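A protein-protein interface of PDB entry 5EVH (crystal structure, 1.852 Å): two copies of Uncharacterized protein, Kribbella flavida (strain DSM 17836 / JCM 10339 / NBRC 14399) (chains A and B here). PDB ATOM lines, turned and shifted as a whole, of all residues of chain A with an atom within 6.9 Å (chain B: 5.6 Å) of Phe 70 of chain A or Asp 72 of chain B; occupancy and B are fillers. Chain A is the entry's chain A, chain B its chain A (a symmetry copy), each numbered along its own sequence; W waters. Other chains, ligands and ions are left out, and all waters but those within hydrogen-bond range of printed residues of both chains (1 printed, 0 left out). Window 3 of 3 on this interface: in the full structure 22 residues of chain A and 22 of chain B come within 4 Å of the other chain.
The backbone carbonyl oxygen of Ser 68 of chain A lies within hydrogen-bond range of the backbone NH of Met 79 of chain A, 2.9 Å away.
O of Phe 70 of chain A is in hydrogen-bond range of N of Leu 77 of chain A.
The backbone NH (N) of Thr 75 of chain A lies within hydrogen-bond range of the side-chain carboxylate (OD1) of Asp 72 of chain A.
O of Asp 72 of chain B sits close to N of Ala 8 of chain B, 3.4 Å away.
The backbone NH (N) of Thr 74 of chain B lies within hydrogen-bond range of the side-chain carboxylate (OD1) of Asp 72 of chain B, at 3.1 Å.
OD1 of Asp 72 of chain B lies within hydrogen-bond range of N of Thr 75 of chain B.
OG of Ser 68 of chain A touches CD2 of Leu 77 of chain B (3.7 Å).
CB of Phe 70 of chain A touches CB of Phe 70 of chain B, at 3.2 Å.
Asp 72 of chain B touches Phe 70 of chain A (N to CE1, 3.9 Å).
Phe 70 of chain A touches Thr 75 of chain B (CZ to OG1, 3.6 Å).
Phe 70 of chain A touches Leu 77 of chain B.
Gly 71 of chain A touches Phe 70 of chain B.
Asp 72 of chain A touches Phe 70 of chain B (N to CE1, 3.9 Å).
CZ of Phe 70 of chain B touches OG1 of Thr 75 of chain A, 3.6 Å away.
Phe 70 of chain B touches Leu 77 of chain A (CD2 to CB, 3.8 Å).
Leu 77 of chain B touches Leu 77 of chain A.
Phe 70 of chain A touches five residues of chain B.
Printed residues of chain B within 4 Å of Gly 71 of chain A: Phe 70 (3.6 Å).
Of the printed residues of chain B, Asp 72 of chain A touches Phe 70.
Asp 72 of chain B touches just one residue of chain A: Phe 70 (3.9 Å).
Of the printed residues of chain A, Leu 77 of chain B touches Ser 68, Phe 70, Leu 77 and Leu 78.
Hydrophobic or aromatic side chains of chain B that line the printed part of chain A: Phe 70 and Leu 77.
Among the printed residues, 12 pairs touch across the chains.
Phe 70 of chain B touches its own counterpart, Phe 70 of chain A.
Phe 70 of chain A touches Gly 71 of chain B, and with the chains exchanged Gly 71 of chain A touches Phe 70 of chain B.
Phe 70 of chain A touches Asp 72 of chain B, and with the chains exchanged Asp 72 of chain A touches Phe 70 of chain B.
Phe 70 of chain A touches Leu 77 of chain B, and with the chains exchanged Leu 77 of chain A touches Phe 70 of chain B.
Positions printed for both chains: 8, 9, 70, 71, 72, 75, 76 and 77.
Water W1 bridges the side-chain hydroxyl of Ser 68 of chain A (2.7 Å) and the side-chain hydroxyl of Thr 75 of chain B (2.8 Å).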
ATOM      1  N   ALA A   8      33.944   0.287   2.055  1.00  0.00           N
ATOM      2  CA  ALA A   8      34.576  -0.798   1.312  1.00  0.00           C
ATOM      3  C   ALA A   8      33.613  -1.380   0.293  1.00  0.00           C
ATOM      4  O   ALA A   8      34.025  -1.784  -0.797  1.00  0.00           O
ATOM      5  CB  ALA A   8      35.058  -1.933   2.253  1.00  0.00           C
ATOM      6  N   LEU A   9      32.344  -1.520   0.657  1.00  0.00           N
ATOM      7  CA  LEU A   9      31.390  -2.083  -0.305  1.00  0.00           C
ATOM      8  C   LEU A   9      31.174  -1.124  -1.480  1.00  0.00           C
ATOM      9  O   LEU A   9      31.000  -1.559  -2.623  1.00  0.00           O
ATOM     10  CB  LEU A   9      30.015  -2.362   0.381  1.00  0.00           C
ATOM     11  CG  LEU A   9      28.953  -3.035  -0.554  1.00  0.00           C
ATOM     12  CD1 LEU A   9      29.523  -4.295  -1.205  1.00  0.00           C
ATOM     13  CD2 LEU A   9      27.687  -3.386   0.218  1.00  0.00           C
ATOM     14  N   ALA A  12      34.069  -1.689  -3.733  1.00  0.00           N
ATOM     15  CA  ALA A  12      33.945  -2.991  -4.369  1.00  0.00           C
ATOM     16  C   ALA A  12      32.937  -2.956  -5.505  1.00  0.00           C
ATOM     17  O   ALA A  12      33.197  -3.500  -6.583  1.00  0.00           O
ATOM     18  CB  ALA A  12      33.524  -4.031  -3.299  1.00  0.00           C
ATOM     19  N   SER A  68      24.573 -11.061  -4.078  1.00  0.00           N
ATOM     20  CA  SER A  68      24.620 -10.722  -2.655  1.00  0.00           C
ATOM     21  C   SER A  68      25.849  -9.857  -2.451  1.00  0.00           C
ATOM     22  O   SER A  68      26.856 -10.088  -3.117  1.00  0.00           O
ATOM     23  CB  SER A  68      24.724 -12.018  -1.811  1.00  0.00           C
ATOM     24  OG  SER A  68      24.660 -11.737  -0.412  1.00  0.00           O
ATOM     25  N   ALA A  69      25.753  -8.841  -1.590  1.00  0.00           N
ATOM     26  CA  ALA A  69      26.905  -7.971  -1.354  1.00  0.00           C
ATOM     27  C   ALA A  69      26.775  -7.339   0.016  1.00  0.00           C
ATOM     28  O   ALA A  69      25.713  -6.785   0.311  1.00  0.00           O
ATOM     29  CB  ALA A  69      26.970  -6.862  -2.429  1.00  0.00           C
ATOM     30  N   PHE A  70      27.865  -7.337   0.815  1.00  0.00           N
ATOM     31  CA  PHE A  70      27.854  -6.814   2.158  1.00  0.00           C
ATOM     32  C   PHE A  70      29.214  -6.210   2.385  1.00  0.00           C
ATOM     33  O   PHE A  70      30.194  -6.598   1.733  1.00  0.00           O
ATOM     34  CB  PHE A  70      27.678  -7.924   3.215  1.00  0.00           C
ATOM     35  CG  PHE A  70      26.308  -8.526   3.255  1.00  0.00           C
ATOM     36  CD1 PHE A  70      25.288  -7.911   4.020  1.00  0.00           C
ATOM     37  CD2 PHE A  70      26.023  -9.722   2.590  1.00  0.00           C
ATOM     38  CE1 PHE A  70      24.037  -8.518   4.123  1.00  0.00           C
ATOM     39  CE2 PHE A  70      24.756 -10.333   2.686  1.00  0.00           C
ATOM     40  CZ  PHE A  70      23.745  -9.670   3.460  1.00  0.00           C
ATOM     41  N   GLY A  71      29.301  -5.275   3.308  1.00  0.00           N
ATOM     42  CA  GLY A  71      30.649  -4.929   3.734  1.00  0.00           C
ATOM     43  C   GLY A  71      30.626  -4.034   4.951  1.00  0.00           C
ATOM     44  O   GLY A  71      29.569  -3.721   5.503  1.00  0.00           O
ATOM     45  N   ASP A  72      31.819  -3.696   5.421  1.00  0.00           N
ATOM     46  CA  ASP A  72      31.955  -2.712   6.507  1.00  0.00           C
ATOM     47  C   ASP A  72      32.972  -1.649   6.099  1.00  0.00           C
ATOM     48  O   ASP A  72      33.138  -1.346   4.914  1.00  0.00           O
ATOM     49  CB  ASP A  72      32.342  -3.399   7.829  1.00  0.00           C
ATOM     50  CG  ASP A  72      33.628  -4.251   7.732  1.00  0.00           C
ATOM     51  OD1 ASP A  72      34.508  -4.027   6.856  1.00  0.00           O
ATOM     52  OD2 ASP A  72      33.806  -5.171   8.580  1.00  0.00           O
ATOM     53  N   THR A  75      36.277  -4.009   4.677  1.00  0.00           N
ATOM     54  CA  THR A  75      36.203  -5.230   3.871  1.00  0.00           C
ATOM     55  C   THR A  75      34.828  -5.346   3.271  1.00  0.00           C
ATOM     56  O   THR A  75      33.847  -4.782   3.788  1.00  0.00           O
ATOM     57  CB  THR A  75      36.472  -6.533   4.653  1.00  0.00           C
ATOM     58  OG1 THR A  75      35.472  -6.706   5.649  1.00  0.00           O
ATOM     59  CG2 THR A  75      37.904  -6.551   5.278  1.00  0.00           C
ATOM     60  N   ALA A  76      34.759  -6.124   2.185  1.00  0.00           N
ATOM     61  CA  ALA A  76      33.518  -6.350   1.501  1.00  0.00           C
ATOM     62  C   ALA A  76      33.519  -7.788   1.023  1.00  0.00           C
ATOM     63  O   ALA A  76      34.573  -8.389   0.754  1.00  0.00           O
ATOM     64  CB  ALA A  76      33.322  -5.361   0.306  1.00  0.00           C
ATOM     65  N   LEU A  77      32.316  -8.311   0.849  1.00  0.00           N
ATOM     66  CA  LEU A  77      32.139  -9.673   0.394  1.00  0.00           C
ATOM     67  C   LEU A  77      31.000  -9.648  -0.623  1.00  0.00           C
ATOM     68  O   LEU A  77      29.904  -9.130  -0.338  1.00  0.00           O
ATOM     69  CB  LEU A  77      31.814 -10.579   1.615  1.00  0.00           C
ATOM     70  CG  LEU A  77      31.803 -12.078   1.357  1.00  0.00           C
ATOM     71  CD1 LEU A  77      33.225 -12.573   0.899  1.00  0.00           C
ATOM     72  CD2 LEU A  77      31.372 -12.833   2.668  1.00  0.00           C
ATOM     73  N   LEU A  78      31.242 -10.181  -1.809  1.00  0.00           N
ATOM     74  CA  LEU A  78      30.141 -10.197  -2.765  1.00  0.00           C
ATOM     75  C   LEU A  78      30.150 -11.464  -3.594  1.00  0.00           C
ATOM     76  O   LEU A  78      31.171 -12.164  -3.713  1.00  0.00           O
ATOM     77  CB  LEU A  78      30.169  -9.028  -3.695  1.00  0.00           C
ATOM     78  CG  LEU A  78      31.455  -8.584  -4.269  1.00  0.00           C
ATOM     79  CD1 LEU A  78      31.309  -8.978  -5.678  1.00  0.00           C
ATOM     80  CD2 LEU A  78      31.357  -7.110  -4.208  1.00  0.00           C
ATOM     81  N   MET A  79      28.959 -11.777  -4.097  1.00  0.00           N
ATOM     82  CA  MET A  79      28.809 -12.972  -4.949  1.00  0.00           C
ATOM     83  C   MET A  79      27.979 -12.514  -6.151  1.00  0.00           C
ATOM     84  O   MET A  79      26.976 -11.773  -5.983  1.00  0.00           O
ATOM     85  CB  MET A  79      28.114 -14.076  -4.200  1.00  0.00           C
ATOM     86  CG  MET A  79      27.923 -15.305  -5.157  1.00  0.00           C
ATOM     87  SD  MET A  79      26.998 -16.813  -4.287  1.00  0.00           S
ATOM     88  CE  MET A  79      28.440 -17.370  -2.991  1.00  0.00           C
ATOM     89  N   SER B   5      19.479  -6.762  13.094  1.00  0.00           N
ATOM     90  CA  SER B   5      19.278  -8.224  13.183  1.00  0.00           C
ATOM     91  C   SER B   5      20.397  -9.024  12.520  1.00  0.00           C
ATOM     92  O   SER B   5      20.842  -8.770  11.382  1.00  0.00           O
ATOM     93  CB  SER B   5      17.956  -8.683  12.572  1.00  0.00           C
ATOM     94  OG  SER B   5      17.877 -10.106  12.490  1.00  0.00           O
ATOM     95  N   THR B   6      20.822 -10.020  13.291  1.00  0.00           N
ATOM     96  CA  THR B   6      21.897 -10.940  12.956  1.00  0.00           C
ATOM     97  C   THR B   6      21.360 -12.334  12.701  1.00  0.00           C
ATOM     98  O   THR B   6      22.149 -13.291  12.710  1.00  0.00           O
ATOM     99  CB  THR B   6      22.903 -10.997  14.125  1.00  0.00           C
ATOM    100  OG1 THR B   6      22.173 -11.374  15.320  1.00  0.00           O
ATOM    101  CG2 THR B   6      23.586  -9.614  14.377  1.00  0.00           C
ATOM    102  N   ALA B   7      20.031 -12.491  12.538  1.00  0.00           N
ATOM    103  CA  ALA B   7      19.441 -13.827  12.613  1.00  0.00           C
ATOM    104  C   ALA B   7      20.019 -14.749  11.542  1.00  0.00           C
ATOM    105  O   ALA B   7      20.381 -15.911  11.812  1.00  0.00           O
ATOM    106  CB  ALA B   7      17.906 -13.743  12.472  1.00  0.00           C
ATOM    107  N   ALA B   8      20.069 -14.279  10.295  1.00  0.00           N
ATOM    108  CA  ALA B   8      20.480 -15.202   9.243  1.00  0.00           C
ATOM    109  C   ALA B   8      21.941 -15.580   9.405  1.00  0.00           C
ATOM    110  O   ALA B   8      22.328 -16.716   9.120  1.00  0.00           O
ATOM    111  CB  ALA B   8      20.271 -14.595   7.832  1.00  0.00           C
ATOM    112  N   LEU B   9      22.786 -14.623   9.769  1.00  0.00           N
ATOM    113  CA  LEU B   9      24.206 -14.957   9.930  1.00  0.00           C
ATOM    114  C   LEU B   9      24.411 -15.897  11.124  1.00  0.00           C
ATOM    115  O   LEU B   9      25.270 -16.783  11.087  1.00  0.00           O
ATOM    116  CB  LEU B   9      25.055 -13.666  10.151  1.00  0.00           C
ATOM    117  CG  LEU B   9      26.597 -13.918  10.258  1.00  0.00           C
ATOM    118  CD1 LEU B   9      27.101 -14.726   9.062  1.00  0.00           C
ATOM    119  CD2 LEU B   9      27.363 -12.605  10.347  1.00  0.00           C
ATOM    120  N   PHE B  70      28.948 -12.048   6.717  1.00  0.00           N
ATOM    121  CA  PHE B  70      28.091 -10.899   6.868  1.00  0.00           C
ATOM    122  C   PHE B  70      26.680 -11.406   6.728  1.00  0.00           C
ATOM    123  O   PHE B  70      26.443 -12.448   6.101  1.00  0.00           O
ATOM    124  CB  PHE B  70      28.304  -9.861   5.747  1.00  0.00           C
ATOM    125  CG  PHE B  70      29.601  -9.119   5.832  1.00  0.00           C
ATOM    126  CD1 PHE B  70      29.703  -7.966   6.646  1.00  0.00           C
ATOM    127  CD2 PHE B  70      30.711  -9.511   5.078  1.00  0.00           C
ATOM    128  CE1 PHE B  70      30.887  -7.228   6.660  1.00  0.00           C
ATOM    129  CE2 PHE B  70      31.911  -8.772   5.096  1.00  0.00           C
ATOM    130  CZ  PHE B  70      31.978  -7.616   5.947  1.00  0.00           C
ATOM    131  N   GLY B  71      25.733 -10.682   7.286  1.00  0.00           N
ATOM    132  CA  GLY B  71      24.371 -11.002   6.884  1.00  0.00           C
ATOM    133  C   GLY B  71      23.392  -9.968   7.390  1.00  0.00           C
ATOM    134  O   GLY B  71      23.769  -8.971   8.009  1.00  0.00           O
ATOM    135  N   ASP B  72      22.130 -10.173   7.040  1.00  0.00           N
ATOM    136  CA  ASP B  72      21.048  -9.335   7.581  1.00  0.00           C
ATOM    137  C   ASP B  72      19.945 -10.233   8.137  1.00  0.00           C
ATOM    138  O   ASP B  72      20.202 -11.350   8.594  1.00  0.00           O
ATOM    139  CB  ASP B  72      20.514  -8.364   6.513  1.00  0.00           C
ATOM    140  CG  ASP B  72      20.034  -9.066   5.222  1.00  0.00           C
ATOM    141  OD1 ASP B  72      19.664 -10.271   5.220  1.00  0.00           O
ATOM    142  OD2 ASP B  72      19.984  -8.392   4.154  1.00  0.00           O
ATOM    143  N   ALA B  73      18.704  -9.762   8.098  1.00  0.00           N
ATOM    144  CA  ALA B  73      17.659 -10.481   8.792  1.00  0.00           C
ATOM    145  C   ALA B  73      17.365 -11.806   8.101  1.00  0.00           C
ATOM    146  O   ALA B  73      16.990 -12.779   8.771  1.00  0.00           O
ATOM    147  CB  ALA B  73      16.407  -9.610   8.860  1.00  0.00           C
ATOM    148  N   THR B  74      17.543 -11.880   6.765  1.00  0.00           N
ATOM    149  CA  THR B  74      17.129 -13.087   6.064  1.00  0.00           C
ATOM    150  C   THR B  74      18.192 -13.702   5.163  1.00  0.00           C
ATOM    151  O   THR B  74      17.947 -14.793   4.620  1.00  0.00           O
ATOM    152  CB  THR B  74      15.881 -12.809   5.219  1.00  0.00           C
ATOM    153  OG1 THR B  74      16.187 -11.807   4.244  1.00  0.00           O
ATOM    154  CG2 THR B  74      14.666 -12.380   6.137  1.00  0.00           C
ATOM    155  N   THR B  75      19.325 -13.043   4.938  1.00  0.00           N
ATOM    156  CA  THR B  75      20.354 -13.663   4.101  1.00  0.00           C
ATOM    157  C   THR B  75      21.698 -13.487   4.754  1.00  0.00           C
ATOM    158  O   THR B  75      21.908 -12.567   5.563  1.00  0.00           O
ATOM    159  CB  THR B  75      20.459 -13.080   2.675  1.00  0.00           C
ATOM    160  OG1 THR B  75      20.838 -11.711   2.748  1.00  0.00           O
ATOM    161  CG2 THR B  75      19.129 -13.258   1.876  1.00  0.00           C
ATOM    162  N   ALA B  76      22.627 -14.365   4.360  1.00  0.00           N
ATOM    163  CA  ALA B  76      23.964 -14.326   4.877  1.00  0.00           C
ATOM    164  C   ALA B  76      24.901 -14.693   3.743  1.00  0.00           C
ATOM    165  O   ALA B  76      24.544 -15.435   2.812  1.00  0.00           O
ATOM    166  CB  ALA B  76      24.149 -15.293   6.092  1.00  0.00           C
ATOM    167  N   LEU B  77      26.131 -14.221   3.870  1.00  0.00           N
ATOM    168  CA  LEU B  77      27.149 -14.482   2.877  1.00  0.00           C
ATOM    169  C   LEU B  77      28.435 -14.789   3.641  1.00  0.00           C
ATOM    170  O   LEU B  77      28.857 -14.010   4.516  1.00  0.00           O
ATOM    171  CB  LEU B  77      27.297 -13.233   1.961  1.00  0.00           C
ATOM    172  CG  LEU B  77      28.174 -13.401   0.729  1.00  0.00           C
ATOM    173  CD1 LEU B  77      27.576 -14.495  -0.232  1.00  0.00           C
ATOM    174  CD2 LEU B  77      28.283 -12.028  -0.028  1.00  0.00           C
HETATM  175  O   HOH W   1      22.105 -11.403   0.233  1.00  0.00           O
